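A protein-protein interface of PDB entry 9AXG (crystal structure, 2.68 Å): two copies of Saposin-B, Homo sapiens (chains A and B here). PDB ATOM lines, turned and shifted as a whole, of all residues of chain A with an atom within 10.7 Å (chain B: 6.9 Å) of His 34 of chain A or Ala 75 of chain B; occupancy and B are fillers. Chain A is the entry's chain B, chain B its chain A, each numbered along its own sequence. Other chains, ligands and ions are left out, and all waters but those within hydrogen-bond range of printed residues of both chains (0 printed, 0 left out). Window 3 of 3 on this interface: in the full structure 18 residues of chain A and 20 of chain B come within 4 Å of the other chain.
A ring nitrogen (NE2) of His 34 of chain A is in hydrogen-bond range of the backbone carbonyl oxygen of Leu 76 of chain B (2.9 Å).
The backbone carbonyl oxygen (O) of Ala 75 of chain B is in hydrogen-bond range of a ring nitrogen (NE2) of His 34 of chain A (2.6 Å).
The backbone carbonyl oxygen (O) of Cys 74 of chain B sits at hydrogen-bond distance from the backbone NH (N) of Phe 79 of chain B.
SG of Cys 39 of chain A is disulfide-bonded to SG of Cys 50 of chain A.
SG of Cys 80 of chain B forms a disulfide with SG of Cys 7 of chain B.
The side-chain sulfur (SG) of Cys 10 of chain B is disulfide-bonded to the side-chain sulfur (SG) of Cys 74 of chain B (2.0 Å).
Cys 10 of chain B touches Met 13 of chain A.
CE of Met 13 of chain A touches CE2 of Phe 79 of chain B (3.7 Å).
O of Gly 78 of chain B touches CD1 of Leu 31 of chain A (3.3 Å).
Phe 79 of chain B touches Leu 31 of chain A (CE1 to CD2, 3.9 Å).
His 34 of chain A touches Val 77 of chain B (CD2 to O, 3.8 Å).
CD2 of His 34 of chain A touches CA of Gly 78 of chain B (3.5 Å).
Val 77 of chain B touches Val 35 of chain A.
Printed residues of chain B within 4 Å of Leu 31 of chain A: Gly 78 (3.3 Å) and Phe 79 (3.9 Å).
His 34 of chain A touches just these residues of chain B: Ala 75 (2.6 Å), Leu 76 (2.9 Å), Val 77 (3.8 Å) and Gly 78 (3.5 Å).
Of the printed residues of chain B, Val 35 of chain A touches Val 77.
No residue of chain A comes within 4 Å of Lys 71 of chain B.
No residue of chain A comes within 4 Å of Cys 74 of chain B.
Printed residues of chain A within 4 Å of Ala 75 of chain B: His 34.
Leu 76 of chain B touches just one residue of chain A: His 34 (2.9 Å).
Of chain A, only His 34 (3.8 Å) and Val 35 (3.7 Å) come within 4 Å of Val 77 of chain B.
No residue of chain A comes within 4 Å of Asp 81 of chain B.
The nearest residue of chain B that does not touch His 34 of chain A is Cys 74 of chain B (5.5 Å).
The nearest residue of chain A that does not touch Ala 75 of chain B is Arg 41 of chain A (7.0 Å).
The nearest printed residue of chain B that does not touch Met 13 of chain A is Cys 74 of chain B (6.5 Å).
Of the 22 printed residues of chain A, 4 touch a printed residue of chain B.
Printed residues of chain A that touch a printed residue of chain B: Met 13, Leu 31, His 34 and Val 35.
Hydrophobic or aromatic side chains of chain A within 4 Å of the printed part of chain B: Met 13, Leu 31, His 34 and Val 35.
Of the 14 printed residues of chain B, 6 touch a printed residue of chain A.
Along chain B the printed residues that touch a printed residue of chain A span positions 10 to 79.
No position is printed for both chains.
Of the 9 pairs that touch across the chains among the printed residues, none has its exchanged pair printed and touching as well.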
ATOM      1  N   MET A  13      15.451  28.353  -4.489  1.00  0.00           N
ATOM      2  CA  MET A  13      14.679  27.416  -5.292  1.00  0.00           C
ATOM      3  C   MET A  13      14.900  27.641  -6.779  1.00  0.00           C
ATOM      4  O   MET A  13      15.007  26.682  -7.544  1.00  0.00           O
ATOM      5  CB  MET A  13      13.201  27.532  -4.952  1.00  0.00           C
ATOM      6  CG  MET A  13      12.313  26.642  -5.776  1.00  0.00           C
ATOM      7  SD  MET A  13      10.627  26.883  -5.300  1.00  0.00           S
ATOM      8  CE  MET A  13      10.005  27.644  -6.799  1.00  0.00           C
ATOM      9  N   THR A  26      15.376  14.898 -17.851  1.00  0.00           N
ATOM     10  CA  THR A  26      13.952  14.597 -17.777  1.00  0.00           C
ATOM     11  C   THR A  26      13.191  15.547 -16.867  1.00  0.00           C
ATOM     12  O   THR A  26      11.982  15.372 -16.688  1.00  0.00           O
ATOM     13  CB  THR A  26      13.729  13.153 -17.306  1.00  0.00           C
ATOM     14  OG1 THR A  26      13.701  13.118 -15.874  1.00  0.00           O
ATOM     15  CG2 THR A  26      14.826  12.226 -17.816  1.00  0.00           C
ATOM     16  N   PHE A  27      13.866  16.551 -16.296  1.00  0.00           N
ATOM     17  CA  PHE A  27      13.229  17.441 -15.325  1.00  0.00           C
ATOM     18  C   PHE A  27      12.134  18.285 -15.973  1.00  0.00           C
ATOM     19  O   PHE A  27      10.990  18.315 -15.492  1.00  0.00           O
ATOM     20  CB  PHE A  27      14.291  18.336 -14.689  1.00  0.00           C
ATOM     21  CG  PHE A  27      13.736  19.381 -13.763  1.00  0.00           C
ATOM     22  CD1 PHE A  27      13.270  19.035 -12.500  1.00  0.00           C
ATOM     23  CD2 PHE A  27      13.684  20.711 -14.151  1.00  0.00           C
ATOM     24  CE1 PHE A  27      12.761  20.001 -11.639  1.00  0.00           C
ATOM     25  CE2 PHE A  27      13.175  21.689 -13.292  1.00  0.00           C
ATOM     26  CZ  PHE A  27      12.712  21.332 -12.038  1.00  0.00           C
ATOM     27  N   VAL A  28      12.469  18.939 -17.094  1.00  0.00           N
ATOM     28  CA  VAL A  28      11.536  19.794 -17.826  1.00  0.00           C
ATOM     29  C   VAL A  28      10.353  18.987 -18.354  1.00  0.00           C
ATOM     30  O   VAL A  28       9.203  19.432 -18.265  1.00  0.00           O
ATOM     31  CB  VAL A  28      12.285  20.521 -18.961  1.00  0.00           C
ATOM     32  CG1 VAL A  28      11.328  21.184 -19.946  1.00  0.00           C
ATOM     33  CG2 VAL A  28      13.220  21.555 -18.394  1.00  0.00           C
ATOM     34  N   GLN A  29      10.616  17.785 -18.889  1.00  0.00           N
ATOM     35  CA  GLN A  29       9.557  16.928 -19.418  1.00  0.00           C
ATOM     36  C   GLN A  29       8.533  16.579 -18.349  1.00  0.00           C
ATOM     37  O   GLN A  29       7.326  16.766 -18.548  1.00  0.00           O
ATOM     38  CB  GLN A  29      10.147  15.634 -19.967  1.00  0.00           C
ATOM     39  CG  GLN A  29      11.228  15.792 -20.970  1.00  0.00           C
ATOM     40  CD  GLN A  29      11.730  14.448 -21.426  1.00  0.00           C
ATOM     41  OE1 GLN A  29      10.942  13.569 -21.773  1.00  0.00           O
ATOM     42  NE2 GLN A  29      13.046  14.275 -21.422  1.00  0.00           N
ATOM     43  N   ALA A  30       9.009  16.095 -17.198  1.00  0.00           N
ATOM     44  CA  ALA A  30       8.111  15.684 -16.126  1.00  0.00           C
ATOM     45  C   ALA A  30       7.352  16.877 -15.567  1.00  0.00           C
ATOM     46  O   ALA A  30       6.153  16.769 -15.268  1.00  0.00           O
ATOM     47  CB  ALA A  30       8.907  14.978 -15.029  1.00  0.00           C
ATOM     48  N   LEU A  31       8.020  18.037 -15.478  1.00  0.00           N
ATOM     49  CA  LEU A  31       7.357  19.242 -14.990  1.00  0.00           C
ATOM     50  C   LEU A  31       6.240  19.699 -15.930  1.00  0.00           C
ATOM     51  O   LEU A  31       5.121  19.969 -15.478  1.00  0.00           O
ATOM     52  CB  LEU A  31       8.378  20.356 -14.783  1.00  0.00           C
ATOM     53  CG  LEU A  31       7.827  21.546 -13.997  1.00  0.00           C
ATOM     54  CD1 LEU A  31       7.548  21.132 -12.589  1.00  0.00           C
ATOM     55  CD2 LEU A  31       8.811  22.683 -14.004  1.00  0.00           C
ATOM     56  N   VAL A  32       6.509  19.767 -17.241  1.00  0.00           N
ATOM     57  CA  VAL A  32       5.452  20.211 -18.156  1.00  0.00           C
ATOM     58  C   VAL A  32       4.378  19.144 -18.324  1.00  0.00           C
ATOM     59  O   VAL A  32       3.215  19.479 -18.579  1.00  0.00           O
ATOM     60  CB  VAL A  32       6.002  20.680 -19.524  1.00  0.00           C
ATOM     61  CG1 VAL A  32       7.155  21.643 -19.350  1.00  0.00           C
ATOM     62  CG2 VAL A  32       6.412  19.506 -20.416  1.00  0.00           C
ATOM     63  N   GLU A  33       4.716  17.862 -18.140  1.00  0.00           N
ATOM     64  CA  GLU A  33       3.693  16.822 -18.168  1.00  0.00           C
ATOM     65  C   GLU A  33       2.758  16.953 -16.974  1.00  0.00           C
ATOM     66  O   GLU A  33       1.536  16.786 -17.111  1.00  0.00           O
ATOM     67  CB  GLU A  33       4.344  15.439 -18.195  1.00  0.00           C
ATOM     68  N   HIS A  34       3.311  17.298 -15.801  1.00  0.00           N
ATOM     69  CA  HIS A  34       2.469  17.482 -14.626  1.00  0.00           C
ATOM     70  C   HIS A  34       1.619  18.741 -14.738  1.00  0.00           C
ATOM     71  O   HIS A  34       0.474  18.761 -14.269  1.00  0.00           O
ATOM     72  CB  HIS A  34       3.313  17.529 -13.357  1.00  0.00           C
ATOM     73  CG  HIS A  34       2.491  17.673 -12.117  1.00  0.00           C
ATOM     74  ND1 HIS A  34       1.879  16.600 -11.507  1.00  0.00           N
ATOM     75  CD2 HIS A  34       2.130  18.766 -11.403  1.00  0.00           C
ATOM     76  CE1 HIS A  34       1.196  17.021 -10.459  1.00  0.00           C
ATOM     77  NE2 HIS A  34       1.335  18.333 -10.370  1.00  0.00           N
ATOM     78  N   VAL A  35       2.164  19.804 -15.335  1.00  0.00           N
ATOM     79  CA  VAL A  35       1.383  21.027 -15.513  1.00  0.00           C
ATOM     80  C   VAL A  35       0.256  20.806 -16.526  1.00  0.00           C
ATOM     81  O   VAL A  35      -0.864  21.305 -16.351  1.00  0.00           O
ATOM     82  CB  VAL A  35       2.314  22.193 -15.897  1.00  0.00           C
ATOM     83  CG1 VAL A  35       1.528  23.442 -16.252  1.00  0.00           C
ATOM     84  CG2 VAL A  35       3.244  22.505 -14.741  1.00  0.00           C
ATOM     85  N   LYS A  36       0.513  20.018 -17.573  1.00  0.00           N
ATOM     86  CA  LYS A  36      -0.551  19.682 -18.517  1.00  0.00           C
ATOM     87  C   LYS A  36      -1.623  18.801 -17.886  1.00  0.00           C
ATOM     88  O   LYS A  36      -2.812  18.975 -18.187  1.00  0.00           O
ATOM     89  CB  LYS A  36       0.042  18.998 -19.744  1.00  0.00           C
ATOM     90  CG  LYS A  36       0.726  19.954 -20.691  1.00  0.00           C
ATOM     91  CD  LYS A  36       1.061  19.266 -21.986  1.00  0.00           C
ATOM     92  CE  LYS A  36       2.096  20.043 -22.744  1.00  0.00           C
ATOM     93  NZ  LYS A  36       1.958  19.800 -24.199  1.00  0.00           N
ATOM     94  N   GLU A  37      -1.232  17.872 -17.005  1.00  0.00           N
ATOM     95  CA  GLU A  37      -2.227  17.103 -16.259  1.00  0.00           C
ATOM     96  C   GLU A  37      -3.030  17.988 -15.312  1.00  0.00           C
ATOM     97  O   GLU A  37      -4.210  17.713 -15.067  1.00  0.00           O
ATOM     98  CB  GLU A  37      -1.557  15.974 -15.475  1.00  0.00           C
ATOM     99  CG  GLU A  37      -1.065  14.810 -16.321  1.00  0.00           C
ATOM    100  CD  GLU A  37      -0.871  13.540 -15.507  1.00  0.00           C
ATOM    101  OE1 GLU A  37      -0.413  13.639 -14.347  1.00  0.00           O
ATOM    102  OE2 GLU A  37      -1.168  12.443 -16.030  1.00  0.00           O
ATOM    103  N   GLU A  38      -2.426  19.057 -14.788  1.00  0.00           N
ATOM    104  CA  GLU A  38      -3.160  19.958 -13.908  1.00  0.00           C
ATOM    105  C   GLU A  38      -4.149  20.834 -14.669  1.00  0.00           C
ATOM    106  O   GLU A  38      -5.051  21.405 -14.046  1.00  0.00           O
ATOM    107  CB  GLU A  38      -2.188  20.829 -13.111  1.00  0.00           C
ATOM    108  N   CYS A  39      -4.019  20.936 -15.998  1.00  0.00           N
ATOM    109  CA  CYS A  39      -5.004  21.656 -16.803  1.00  0.00           C
ATOM    110  C   CYS A  39      -6.336  20.927 -16.887  1.00  0.00           C
ATOM    111  O   CYS A  39      -7.348  21.552 -17.226  1.00  0.00           O
ATOM    112  CB  CYS A  39      -4.495  21.875 -18.228  1.00  0.00           C
ATOM    113  SG  CYS A  39      -3.181  23.072 -18.425  1.00  0.00           S
ATOM    114  N   ASP A  40      -6.358  19.625 -16.594  1.00  0.00           N
ATOM    115  CA  ASP A  40      -7.551  18.805 -16.767  1.00  0.00           C
ATOM    116  C   ASP A  40      -8.664  19.143 -15.777  1.00  0.00           C
ATOM    117  O   ASP A  40      -9.814  18.751 -16.008  1.00  0.00           O
ATOM    118  CB  ASP A  40      -7.161  17.328 -16.659  1.00  0.00           C
ATOM    119  CG  ASP A  40      -6.561  16.784 -17.951  1.00  0.00           C
ATOM    120  OD1 ASP A  40      -6.799  17.381 -19.023  1.00  0.00           O
ATOM    121  OD2 ASP A  40      -5.827  15.774 -17.889  1.00  0.00           O
ATOM    122  N   ARG A  41      -8.357  19.882 -14.705  1.00  0.00           N
ATOM    123  CA  ARG A  41      -9.374  20.303 -13.746  1.00  0.00           C
ATOM    124  C   ARG A  41     -10.305  21.368 -14.315  1.00  0.00           C
ATOM    125  O   ARG A  41     -11.384  21.593 -13.755  1.00  0.00           O
ATOM    126  CB  ARG A  41      -8.699  20.820 -12.473  1.00  0.00           C
ATOM    127  CG  ARG A  41      -7.561  19.937 -11.982  1.00  0.00           C
ATOM    128  CD  ARG A  41      -6.998  20.425 -10.661  1.00  0.00           C
ATOM    129  NE  ARG A  41      -5.961  19.531 -10.161  1.00  0.00           N
ATOM    130  CZ  ARG A  41      -5.979  18.952  -8.968  1.00  0.00           C
ATOM    131  NH1 ARG A  41      -6.966  19.162  -8.110  1.00  0.00           N
ATOM    132  NH2 ARG A  41      -4.983  18.138  -8.626  1.00  0.00           N
ATOM    133  N   ALA A  47      -9.485  22.585 -21.128  1.00  0.00           N
ATOM    134  CA  ALA A  47      -8.329  21.862 -20.610  1.00  0.00           C
ATOM    135  C   ALA A  47      -7.297  21.659 -21.708  1.00  0.00           C
ATOM    136  O   ALA A  47      -6.093  21.801 -21.475  1.00  0.00           O
ATOM    137  CB  ALA A  47      -8.757  20.513 -20.030  1.00  0.00           C
ATOM    138  N   CYS A  50      -5.707  24.974 -22.336  1.00  0.00           N
ATOM    139  CA  CYS A  50      -4.673  25.154 -21.320  1.00  0.00           C
ATOM    140  C   CYS A  50      -3.415  24.358 -21.648  1.00  0.00           C
ATOM    141  O   CYS A  50      -2.291  24.874 -21.535  1.00  0.00           O
ATOM    142  CB  CYS A  50      -5.233  24.727 -19.963  1.00  0.00           C
ATOM    143  SG  CYS A  50      -4.106  24.884 -18.565  1.00  0.00           S
ATOM    144  N   LYS A  51      -3.596  23.104 -22.078  1.00  0.00           N
ATOM    145  CA  LYS A  51      -2.477  22.218 -22.383  1.00  0.00           C
ATOM    146  C   LYS A  51      -1.657  22.736 -23.560  1.00  0.00           C
ATOM    147  O   LYS A  51      -0.422  22.756 -23.504  1.00  0.00           O
ATOM    148  CB  LYS A  51      -3.001  20.807 -22.676  1.00  0.00           C
ATOM    149  CG  LYS A  51      -3.306  19.944 -21.445  1.00  0.00           C
ATOM    150  CD  LYS A  51      -4.328  18.844 -21.776  1.00  0.00           C
ATOM    151  CE  LYS A  51      -4.070  17.548 -21.003  1.00  0.00           C
ATOM    152  NZ  LYS A  51      -4.176  16.338 -21.875  1.00  0.00           N
ATOM    153  N   ILE A  54       0.283  25.792 -22.724  1.00  0.00           N
ATOM    154  CA  ILE A  54       1.534  25.372 -22.097  1.00  0.00           C
ATOM    155  C   ILE A  54       2.528  24.906 -23.162  1.00  0.00           C
ATOM    156  O   ILE A  54       3.720  25.232 -23.101  1.00  0.00           O
ATOM    157  CB  ILE A  54       1.256  24.289 -21.028  1.00  0.00           C
ATOM    158  CG1 ILE A  54       1.046  24.881 -19.623  1.00  0.00           C
ATOM    159  CG2 ILE A  54       2.380  23.263 -20.935  1.00  0.00           C
ATOM    160  CD1 ILE A  54       0.145  26.096 -19.481  1.00  0.00           C
ATOM    161  N   SER A  58       6.021  26.909 -23.478  1.00  0.00           N
ATOM    162  CA  SER A  58       7.020  26.361 -22.563  1.00  0.00           C
ATOM    163  C   SER A  58       8.432  26.706 -23.012  1.00  0.00           C
ATOM    164  O   SER A  58       9.338  26.790 -22.179  1.00  0.00           O
ATOM    165  CB  SER A  58       6.883  24.849 -22.450  1.00  0.00           C
ATOM    166  OG  SER A  58       7.217  24.234 -23.679  1.00  0.00           O
ATOM    167  N   CYS B   7      12.202  20.158  -4.596  1.00  0.00           N
ATOM    168  CA  CYS B   7      11.023  19.829  -3.795  1.00  0.00           C
ATOM    169  C   CYS B   7      11.123  20.395  -2.380  1.00  0.00           C
ATOM    170  O   CYS B   7      10.183  21.030  -1.883  1.00  0.00           O
ATOM    171  CB  CYS B   7      10.844  18.308  -3.755  1.00  0.00           C
ATOM    172  SG  CYS B   7       9.510  17.708  -2.683  1.00  0.00           S
ATOM    173  N   CYS B  10      10.881  24.160  -2.464  1.00  0.00           N
ATOM    174  CA  CYS B  10       9.504  24.588  -2.665  1.00  0.00           C
ATOM    175  C   CYS B  10       8.693  24.500  -1.384  1.00  0.00           C
ATOM    176  O   CYS B  10       7.873  25.384  -1.119  1.00  0.00           O
ATOM    177  CB  CYS B  10       8.841  23.750  -3.752  1.00  0.00           C
ATOM    178  SG  CYS B  10       7.118  24.225  -4.061  1.00  0.00           S
ATOM    179  N   PRO B  70       1.943  22.769   2.486  1.00  0.00           N
ATOM    180  CA  PRO B  70       2.916  23.142   1.435  1.00  0.00           C
ATOM    181  C   PRO B  70       3.369  22.011   0.516  1.00  0.00           C
ATOM    182  O   PRO B  70       3.638  22.273  -0.668  1.00  0.00           O
ATOM    183  CB  PRO B  70       4.093  23.699   2.250  1.00  0.00           C
ATOM    184  CG  PRO B  70       3.468  24.196   3.499  1.00  0.00           C
ATOM    185  CD  PRO B  70       2.377  23.236   3.815  1.00  0.00           C
ATOM    186  N   LYS B  71       3.476  20.773   1.013  1.00  0.00           N
ATOM    187  CA  LYS B  71       3.870  19.663   0.149  1.00  0.00           C
ATOM    188  C   LYS B  71       2.793  19.363  -0.885  1.00  0.00           C
ATOM    189  O   LYS B  71       3.107  19.009  -2.027  1.00  0.00           O
ATOM    190  CB  LYS B  71       4.183  18.416   0.978  1.00  0.00           C
ATOM    191  N   GLU B  72       1.518  19.521  -0.509  1.00  0.00           N
ATOM    192  CA  GLU B  72       0.431  19.422  -1.477  1.00  0.00           C
ATOM    193  C   GLU B  72       0.505  20.534  -2.515  1.00  0.00           C
ATOM    194  O   GLU B  72       0.242  20.286  -3.697  1.00  0.00           O
ATOM    195  CB  GLU B  72      -0.920  19.466  -0.769  1.00  0.00           C
ATOM    196  CG  GLU B  72      -1.503  18.118  -0.402  1.00  0.00           C
ATOM    197  CD  GLU B  72      -2.487  18.224   0.747  1.00  0.00           C
ATOM    198  OE1 GLU B  72      -3.287  19.186   0.746  1.00  0.00           O
ATOM    199  OE2 GLU B  72      -2.462  17.350   1.645  1.00  0.00           O
ATOM    200  N   ILE B  73       0.862  21.758  -2.092  1.00  0.00           N
ATOM    201  CA  ILE B  73       1.027  22.874  -3.029  1.00  0.00           C
ATOM    202  C   ILE B  73       2.115  22.551  -4.047  1.00  0.00           C
ATOM    203  O   ILE B  73       1.919  22.697  -5.259  1.00  0.00           O
ATOM    204  CB  ILE B  73       1.361  24.182  -2.283  1.00  0.00           C
ATOM    205  CG1 ILE B  73       0.288  24.579  -1.265  1.00  0.00           C
ATOM    206  CG2 ILE B  73       1.557  25.325  -3.278  1.00  0.00           C
ATOM    207  CD1 ILE B  73      -1.024  24.979  -1.865  1.00  0.00           C
ATOM    208  N   CYS B  74       3.255  22.049  -3.572  1.00  0.00           N
ATOM    209  CA  CYS B  74       4.348  21.750  -4.486  1.00  0.00           C
ATOM    210  C   CYS B  74       4.085  20.503  -5.316  1.00  0.00           C
ATOM    211  O   CYS B  74       4.585  20.401  -6.441  1.00  0.00           O
ATOM    212  CB  CYS B  74       5.643  21.604  -3.707  1.00  0.00           C
ATOM    213  SG  CYS B  74       6.032  23.071  -2.770  1.00  0.00           S
ATOM    214  N   ALA B  75       3.305  19.561  -4.789  1.00  0.00           N
ATOM    215  CA  ALA B  75       2.852  18.438  -5.594  1.00  0.00           C
ATOM    216  C   ALA B  75       1.927  18.913  -6.700  1.00  0.00           C
ATOM    217  O   ALA B  75       1.993  18.412  -7.825  1.00  0.00           O
ATOM    218  CB  ALA B  75       2.149  17.412  -4.709  1.00  0.00           C
ATOM    219  N   LEU B  76       1.076  19.896  -6.401  1.00  0.00           N
ATOM    220  CA  LEU B  76       0.168  20.431  -7.407  1.00  0.00           C
ATOM    221  C   LEU B  76       0.927  21.211  -8.472  1.00  0.00           C
ATOM    222  O   LEU B  76       0.647  21.070  -9.666  1.00  0.00           O
ATOM    223  CB  LEU B  76      -0.894  21.311  -6.742  1.00  0.00           C
ATOM    224  N   VAL B  77       1.895  22.030  -8.059  1.00  0.00           N
ATOM    225  CA  VAL B  77       2.631  22.867  -9.003  1.00  0.00           C
ATOM    226  C   VAL B  77       3.596  22.019  -9.833  1.00  0.00           C
ATOM    227  O   VAL B  77       3.739  22.218 -11.048  1.00  0.00           O
ATOM    228  CB  VAL B  77       3.331  24.006  -8.236  1.00  0.00           C
ATOM    229  CG1 VAL B  77       4.538  24.528  -8.972  1.00  0.00           C
ATOM    230  CG2 VAL B  77       2.347  25.136  -7.966  1.00  0.00           C
ATOM    231  N   GLY B  78       4.253  21.046  -9.210  1.00  0.00           N
ATOM    232  CA  GLY B  78       5.019  20.085  -9.978  1.00  0.00           C
ATOM    233  C   GLY B  78       6.439  19.891  -9.497  1.00  0.00           C
ATOM    234  O   GLY B  78       7.193  19.100 -10.067  1.00  0.00           O
ATOM    235  N   PHE B  79       6.825  20.620  -8.457  1.00  0.00           N
ATOM    236  CA  PHE B  79       8.187  20.532  -7.954  1.00  0.00           C
ATOM    237  C   PHE B  79       8.390  19.381  -6.980  1.00  0.00           C
ATOM    238  O   PHE B  79       9.543  19.066  -6.663  1.00  0.00           O
ATOM    239  CB  PHE B  79       8.570  21.856  -7.299  1.00  0.00           C
ATOM    240  CG  PHE B  79       8.613  23.011  -8.258  1.00  0.00           C
ATOM    241  CD1 PHE B  79       9.273  22.900  -9.467  1.00  0.00           C
ATOM    242  CD2 PHE B  79       7.977  24.197  -7.961  1.00  0.00           C
ATOM    243  CE1 PHE B  79       9.314  23.957 -10.350  1.00  0.00           C
ATOM    244  CE2 PHE B  79       8.014  25.262  -8.841  1.00  0.00           C
ATOM    245  CZ  PHE B  79       8.679  25.141 -10.037  1.00  0.00           C
ATOM    246  N   CYS B  80       7.316  18.745  -6.508  1.00  0.00           N
ATOM    247  CA  CYS B  80       7.403  17.607  -5.604  1.00  0.00           C
ATOM    248  C   CYS B  80       6.635  16.416  -6.172  1.00  0.00           C
ATOM    249  O   CYS B  80       5.605  16.584  -6.838  1.00  0.00           O
ATOM    250  CB  CYS B  80       6.858  17.948  -4.209  1.00  0.00           C
ATOM    251  SG  CYS B  80       7.961  18.929  -3.163  1.00  0.00           S
ATOM    252  N   ASP B  81       7.148  15.218  -5.870  1.00  0.00           N
ATOM    253  CA  ASP B  81       6.634  13.928  -6.351  1.00  0.00           C
ATOM    254  C   ASP B  81       6.545  13.869  -7.876  1.00  0.00           C
ATOM    255  O   ASP B  81       5.535  13.432  -8.430  1.00  0.00           O
ATOM    256  CB  ASP B  81       5.263  13.611  -5.728  1.00  0.00           C
